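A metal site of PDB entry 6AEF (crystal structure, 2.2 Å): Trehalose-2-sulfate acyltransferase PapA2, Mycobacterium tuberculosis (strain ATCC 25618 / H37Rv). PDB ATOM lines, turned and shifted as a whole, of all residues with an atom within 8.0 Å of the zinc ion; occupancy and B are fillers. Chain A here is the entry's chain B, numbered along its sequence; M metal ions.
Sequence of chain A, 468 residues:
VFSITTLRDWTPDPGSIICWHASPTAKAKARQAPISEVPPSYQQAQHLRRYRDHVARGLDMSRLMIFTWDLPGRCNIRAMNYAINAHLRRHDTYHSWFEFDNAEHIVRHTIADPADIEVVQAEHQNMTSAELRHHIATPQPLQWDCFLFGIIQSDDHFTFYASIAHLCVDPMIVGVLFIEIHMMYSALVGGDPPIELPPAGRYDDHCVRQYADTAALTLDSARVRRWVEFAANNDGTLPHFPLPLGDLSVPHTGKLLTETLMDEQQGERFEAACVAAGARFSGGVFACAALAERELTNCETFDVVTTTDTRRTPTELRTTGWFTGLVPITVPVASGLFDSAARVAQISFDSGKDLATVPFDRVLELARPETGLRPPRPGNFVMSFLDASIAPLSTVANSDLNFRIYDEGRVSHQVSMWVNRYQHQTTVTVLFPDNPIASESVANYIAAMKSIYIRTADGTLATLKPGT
The backbone NH (N) of Ala 122 lies within hydrogen-bond range of the backbone carbonyl oxygen (O) of Cys 19 (2.9 Å).
O of Phe 149 sits close to SG of Cys 19, 3.8 Å away.
SG of Cys 19 lies close to OH of Tyr 161.
N of His 124 sits at hydrogen-bond distance from O of Ile 17 (2.9 Å).
The backbone carbonyl oxygen (O) of His 21 sits at hydrogen-bond distance from the backbone NH (N) of Val 120.
The backbone carbonyl oxygen of His 135 is in hydrogen-bond range of the side-chain hydroxyl of Thr 138, at 2.6 Å.
The zinc ion is bound by NE2 of His 21.
The zinc ion is bound by NE2 of His 135, 2.0 Å away.
A ring nitrogen (NE2) of His 124 is bound to the zinc ion (2.2 Å).
The zinc ion is bound by SG of Cys 19 (2.4 Å).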
ATOM      1  N   ILE A  17      33.896 -15.958  -5.654  1.00  0.00           N
ATOM      2  CA  ILE A  17      33.265 -14.874  -4.899  1.00  0.00           C
ATOM      3  C   ILE A  17      33.612 -15.054  -3.417  1.00  0.00           C
ATOM      4  O   ILE A  17      33.170 -16.022  -2.784  1.00  0.00           O
ATOM      5  CB  ILE A  17      31.755 -14.849  -5.137  1.00  0.00           C
ATOM      6  CG1 ILE A  17      31.463 -14.653  -6.636  1.00  0.00           C
ATOM      7  CG2 ILE A  17      31.096 -13.743  -4.322  1.00  0.00           C
ATOM      8  CD1 ILE A  17      30.030 -14.959  -7.038  1.00  0.00           C
ATOM      9  N   ILE A  18      34.414 -14.130  -2.884  1.00  0.00           N
ATOM     10  CA  ILE A  18      34.799 -14.128  -1.474  1.00  0.00           C
ATOM     11  C   ILE A  18      34.138 -12.923  -0.811  1.00  0.00           C
ATOM     12  O   ILE A  18      34.451 -11.777  -1.154  1.00  0.00           O
ATOM     13  CB  ILE A  18      36.324 -14.072  -1.300  1.00  0.00           C
ATOM     14  CG1 ILE A  18      37.009 -15.158  -2.138  1.00  0.00           C
ATOM     15  CG2 ILE A  18      36.709 -14.175   0.180  1.00  0.00           C
ATOM     16  CD1 ILE A  18      36.515 -16.539  -1.862  1.00  0.00           C
ATOM     17  N   CYS A  19      33.265 -13.186   0.167  1.00  0.00           N
ATOM     18  CA  CYS A  19      32.339 -12.170   0.651  1.00  0.00           C
ATOM     19  C   CYS A  19      32.384 -12.107   2.175  1.00  0.00           C
ATOM     20  O   CYS A  19      32.414 -13.136   2.853  1.00  0.00           O
ATOM     21  CB  CYS A  19      30.918 -12.469   0.175  1.00  0.00           C
ATOM     22  SG  CYS A  19      29.767 -11.095   0.335  1.00  0.00           S
ATOM     23  N   TRP A  20      32.370 -10.881   2.704  1.00  0.00           N
ATOM     24  CA  TRP A  20      32.467 -10.624   4.140  1.00  0.00           C
ATOM     25  C   TRP A  20      31.082 -10.388   4.735  1.00  0.00           C
ATOM     26  O   TRP A  20      30.392  -9.445   4.345  1.00  0.00           O
ATOM     27  CB  TRP A  20      33.368  -9.435   4.416  1.00  0.00           C
ATOM     28  CG  TRP A  20      34.838  -9.763   4.430  1.00  0.00           C
ATOM     29  CD1 TRP A  20      35.634  -9.930   5.527  1.00  0.00           C
ATOM     30  CD2 TRP A  20      35.682  -9.970   3.297  1.00  0.00           C
ATOM     31  NE1 TRP A  20      36.921 -10.222   5.139  1.00  0.00           N
ATOM     32  CE2 TRP A  20      36.977 -10.246   3.771  1.00  0.00           C
ATOM     33  CE3 TRP A  20      35.466  -9.948   1.908  1.00  0.00           C
ATOM     34  CZ2 TRP A  20      38.045 -10.506   2.929  1.00  0.00           C
ATOM     35  CZ3 TRP A  20      36.526 -10.203   1.071  1.00  0.00           C
ATOM     36  CH2 TRP A  20      37.808 -10.471   1.579  1.00  0.00           C
ATOM     37  N   HIS A  21      30.691 -11.233   5.675  1.00  0.00           N
ATOM     38  CA  HIS A  21      29.435 -11.077   6.403  1.00  0.00           C
ATOM     39  C   HIS A  21      29.748 -10.864   7.877  1.00  0.00           C
ATOM     40  O   HIS A  21      30.730 -11.374   8.400  1.00  0.00           O
ATOM     41  CB  HIS A  21      28.532 -12.305   6.250  1.00  0.00           C
ATOM     42  CG  HIS A  21      28.046 -12.539   4.849  1.00  0.00           C
ATOM     43  ND1 HIS A  21      26.999 -13.398   4.571  1.00  0.00           N
ATOM     44  CD2 HIS A  21      28.455 -12.049   3.663  1.00  0.00           C
ATOM     45  CE1 HIS A  21      26.787 -13.411   3.270  1.00  0.00           C
ATOM     46  NE2 HIS A  21      27.657 -12.601   2.697  1.00  0.00           N
ATOM     47  N   VAL A 120      33.536 -11.432   8.557  1.00  0.00           N
ATOM     48  CA  VAL A 120      34.362 -12.599   8.293  1.00  0.00           C
ATOM     49  C   VAL A 120      34.055 -13.031   6.871  1.00  0.00           C
ATOM     50  O   VAL A 120      32.894 -13.001   6.442  1.00  0.00           O
ATOM     51  CB  VAL A 120      34.087 -13.744   9.287  1.00  0.00           C
ATOM     52  CG1 VAL A 120      34.857 -15.001   8.887  1.00  0.00           C
ATOM     53  CG2 VAL A 120      34.478 -13.317  10.674  1.00  0.00           C
ATOM     54  N   ALA A 122      33.821 -15.550   3.581  1.00  0.00           N
ATOM     55  CA  ALA A 122      33.534 -16.912   3.181  1.00  0.00           C
ATOM     56  C   ALA A 122      33.338 -16.914   1.679  1.00  0.00           C
ATOM     57  O   ALA A 122      32.881 -15.932   1.096  1.00  0.00           O
ATOM     58  CB  ALA A 122      32.294 -17.474   3.896  1.00  0.00           C
ATOM     59  N   GLU A 123      33.704 -18.022   1.053  1.00  0.00           N
ATOM     60  CA  GLU A 123      33.468 -18.172  -0.373  1.00  0.00           C
ATOM     61  C   GLU A 123      32.032 -18.606  -0.621  1.00  0.00           C
ATOM     62  O   GLU A 123      31.539 -19.547   0.011  1.00  0.00           O
ATOM     63  CB  GLU A 123      34.446 -19.175  -0.981  1.00  0.00           C
ATOM     64  CG  GLU A 123      34.273 -19.355  -2.490  1.00  0.00           C
ATOM     65  CD  GLU A 123      35.328 -20.231  -3.114  1.00  0.00           C
ATOM     66  OE1 GLU A 123      36.236 -20.687  -2.384  1.00  0.00           O
ATOM     67  OE2 GLU A 123      35.272 -20.463  -4.348  1.00  0.00           O
ATOM     68  N   HIS A 124      31.354 -17.903  -1.539  1.00  0.00           N
ATOM     69  CA  HIS A 124      30.052 -18.332  -2.053  1.00  0.00           C
ATOM     70  C   HIS A 124      30.363 -19.308  -3.178  1.00  0.00           C
ATOM     71  O   HIS A 124      30.482 -18.940  -4.341  1.00  0.00           O
ATOM     72  CB  HIS A 124      29.226 -17.134  -2.521  1.00  0.00           C
ATOM     73  CG  HIS A 124      28.811 -16.207  -1.417  1.00  0.00           C
ATOM     74  ND1 HIS A 124      28.464 -16.653  -0.159  1.00  0.00           N
ATOM     75  CD2 HIS A 124      28.713 -14.858  -1.378  1.00  0.00           C
ATOM     76  CE1 HIS A 124      28.154 -15.605   0.595  1.00  0.00           C
ATOM     77  NE2 HIS A 124      28.297 -14.513  -0.120  1.00  0.00           N
ATOM     78  N   MET A 127      28.072 -19.718  -6.426  1.00  0.00           N
ATOM     79  CA  MET A 127      27.198 -18.591  -6.701  1.00  0.00           C
ATOM     80  C   MET A 127      27.389 -18.126  -8.153  1.00  0.00           C
ATOM     81  O   MET A 127      28.510 -17.853  -8.592  1.00  0.00           O
ATOM     82  CB  MET A 127      27.483 -17.450  -5.729  1.00  0.00           C
ATOM     83  CG  MET A 127      26.687 -16.176  -5.978  1.00  0.00           C
ATOM     84  SD  MET A 127      26.871 -14.947  -4.663  1.00  0.00           S
ATOM     85  CE  MET A 127      25.845 -15.637  -3.379  1.00  0.00           C
ATOM     86  N   LEU A 132      24.625 -13.462  -7.583  1.00  0.00           N
ATOM     87  CA  LEU A 132      25.451 -12.415  -6.975  1.00  0.00           C
ATOM     88  C   LEU A 132      24.787 -11.043  -7.127  1.00  0.00           C
ATOM     89  O   LEU A 132      24.813 -10.237  -6.194  1.00  0.00           O
ATOM     90  CB  LEU A 132      26.843 -12.399  -7.595  1.00  0.00           C
ATOM     91  CG  LEU A 132      27.744 -11.247  -7.154  1.00  0.00           C
ATOM     92  CD1 LEU A 132      28.027 -11.281  -5.649  1.00  0.00           C
ATOM     93  CD2 LEU A 132      29.054 -11.244  -7.949  1.00  0.00           C
ATOM     94  N   HIS A 135      22.272 -11.009  -4.492  1.00  0.00           N
ATOM     95  CA  HIS A 135      22.874 -11.002  -3.158  1.00  0.00           C
ATOM     96  C   HIS A 135      23.379  -9.621  -2.784  1.00  0.00           C
ATOM     97  O   HIS A 135      23.173  -9.163  -1.642  1.00  0.00           O
ATOM     98  CB  HIS A 135      24.019 -12.015  -3.120  1.00  0.00           C
ATOM     99  CG  HIS A 135      24.752 -12.074  -1.812  1.00  0.00           C
ATOM    100  ND1 HIS A 135      24.121 -12.389  -0.621  1.00  0.00           N
ATOM    101  CD2 HIS A 135      26.054 -11.890  -1.502  1.00  0.00           C
ATOM    102  CE1 HIS A 135      25.011 -12.373   0.360  1.00  0.00           C
ATOM    103  NE2 HIS A 135      26.185 -12.075  -0.152  1.00  0.00           N
ATOM    104  N   ILE A 136      24.040  -8.931  -3.716  1.00  0.00           N
ATOM    105  CA  ILE A 136      24.655  -7.656  -3.399  1.00  0.00           C
ATOM    106  C   ILE A 136      23.602  -6.591  -3.099  1.00  0.00           C
ATOM    107  O   ILE A 136      23.901  -5.605  -2.427  1.00  0.00           O
ATOM    108  CB  ILE A 136      25.579  -7.241  -4.566  1.00  0.00           C
ATOM    109  CG1 ILE A 136      26.577  -6.179  -4.114  1.00  0.00           C
ATOM    110  CG2 ILE A 136      24.761  -6.725  -5.773  1.00  0.00           C
ATOM    111  CD1 ILE A 136      27.620  -5.824  -5.184  1.00  0.00           C
ATOM    112  N   THR A 138      20.858  -7.082  -1.266  1.00  0.00           N
ATOM    113  CA  THR A 138      19.997  -7.523  -0.164  1.00  0.00           C
ATOM    114  C   THR A 138      20.024  -6.601   1.049  1.00  0.00           C
ATOM    115  O   THR A 138      19.003  -6.488   1.737  1.00  0.00           O
ATOM    116  CB  THR A 138      20.374  -8.936   0.312  1.00  0.00           C
ATOM    117  OG1 THR A 138      21.788  -9.013   0.565  1.00  0.00           O
ATOM    118  CG2 THR A 138      19.983  -9.983  -0.731  1.00  0.00           C
ATOM    119  N   PHE A 147      25.275  -3.858   5.096  1.00  0.00           N
ATOM    120  CA  PHE A 147      26.417  -3.665   4.224  1.00  0.00           C
ATOM    121  C   PHE A 147      26.987  -5.014   3.826  1.00  0.00           C
ATOM    122  O   PHE A 147      26.867  -5.991   4.559  1.00  0.00           O
ATOM    123  CB  PHE A 147      27.496  -2.814   4.898  1.00  0.00           C
ATOM    124  CG  PHE A 147      27.679  -3.111   6.360  1.00  0.00           C
ATOM    125  CD1 PHE A 147      28.428  -4.220   6.763  1.00  0.00           C
ATOM    126  CD2 PHE A 147      27.103  -2.303   7.324  1.00  0.00           C
ATOM    127  CE1 PHE A 147      28.586  -4.503   8.108  1.00  0.00           C
ATOM    128  CE2 PHE A 147      27.261  -2.585   8.669  1.00  0.00           C
ATOM    129  CZ  PHE A 147      28.002  -3.677   9.062  1.00  0.00           C
ATOM    130  N   LEU A 148      27.602  -5.054   2.652  1.00  0.00           N
ATOM    131  CA  LEU A 148      28.343  -6.213   2.167  1.00  0.00           C
ATOM    132  C   LEU A 148      29.609  -5.711   1.491  1.00  0.00           C
ATOM    133  O   LEU A 148      29.608  -4.661   0.855  1.00  0.00           O
ATOM    134  CB  LEU A 148      27.524  -7.042   1.167  1.00  0.00           C
ATOM    135  CG  LEU A 148      26.310  -7.796   1.705  1.00  0.00           C
ATOM    136  CD1 LEU A 148      25.469  -8.305   0.543  1.00  0.00           C
ATOM    137  CD2 LEU A 148      26.707  -8.949   2.632  1.00  0.00           C
ATOM    138  N   PHE A 149      30.687  -6.470   1.642  1.00  0.00           N
ATOM    139  CA  PHE A 149      31.950  -6.184   0.982  1.00  0.00           C
ATOM    140  C   PHE A 149      32.500  -7.494   0.449  1.00  0.00           C
ATOM    141  O   PHE A 149      32.423  -8.516   1.127  1.00  0.00           O
ATOM    142  CB  PHE A 149      32.957  -5.552   1.948  1.00  0.00           C
ATOM    143  CG  PHE A 149      32.482  -4.282   2.574  1.00  0.00           C
ATOM    144  CD1 PHE A 149      32.700  -3.067   1.968  1.00  0.00           C
ATOM    145  CD2 PHE A 149      31.830  -4.305   3.801  1.00  0.00           C
ATOM    146  CE1 PHE A 149      32.272  -1.889   2.552  1.00  0.00           C
ATOM    147  CE2 PHE A 149      31.395  -3.129   4.397  1.00  0.00           C
ATOM    148  CZ  PHE A 149      31.619  -1.924   3.770  1.00  0.00           C
ATOM    149  N   GLY A 150      33.089  -7.459  -0.738  1.00  0.00           N
ATOM    150  CA  GLY A 150      33.680  -8.697  -1.201  1.00  0.00           C
ATOM    151  C   GLY A 150      34.564  -8.484  -2.404  1.00  0.00           C
ATOM    152  O   GLY A 150      34.819  -7.352  -2.821  1.00  0.00           O
ATOM    153  N   TYR A 161      33.946  -5.213  -4.534  1.00  0.00           N
ATOM    154  CA  TYR A 161      32.619  -4.621  -4.506  1.00  0.00           C
ATOM    155  C   TYR A 161      32.241  -4.234  -3.086  1.00  0.00           C
ATOM    156  O   TYR A 161      32.655  -4.874  -2.110  1.00  0.00           O
ATOM    157  CB  TYR A 161      31.553  -5.556  -5.134  1.00  0.00           C
ATOM    158  CG  TYR A 161      31.308  -6.868  -4.425  1.00  0.00           C
ATOM    159  CD1 TYR A 161      30.456  -6.948  -3.335  1.00  0.00           C
ATOM    160  CD2 TYR A 161      31.895  -8.036  -4.882  1.00  0.00           C
ATOM    161  CE1 TYR A 161      30.218  -8.161  -2.700  1.00  0.00           C
ATOM    162  CE2 TYR A 161      31.670  -9.235  -4.263  1.00  0.00           C
ATOM    163  CZ  TYR A 161      30.839  -9.303  -3.177  1.00  0.00           C
ATOM    164  OH  TYR A 161      30.642 -10.522  -2.576  1.00  0.00           O
HETATM  165 ZN    ZN M   1      27.957 -12.565   0.748  1.00  0.00          ZN
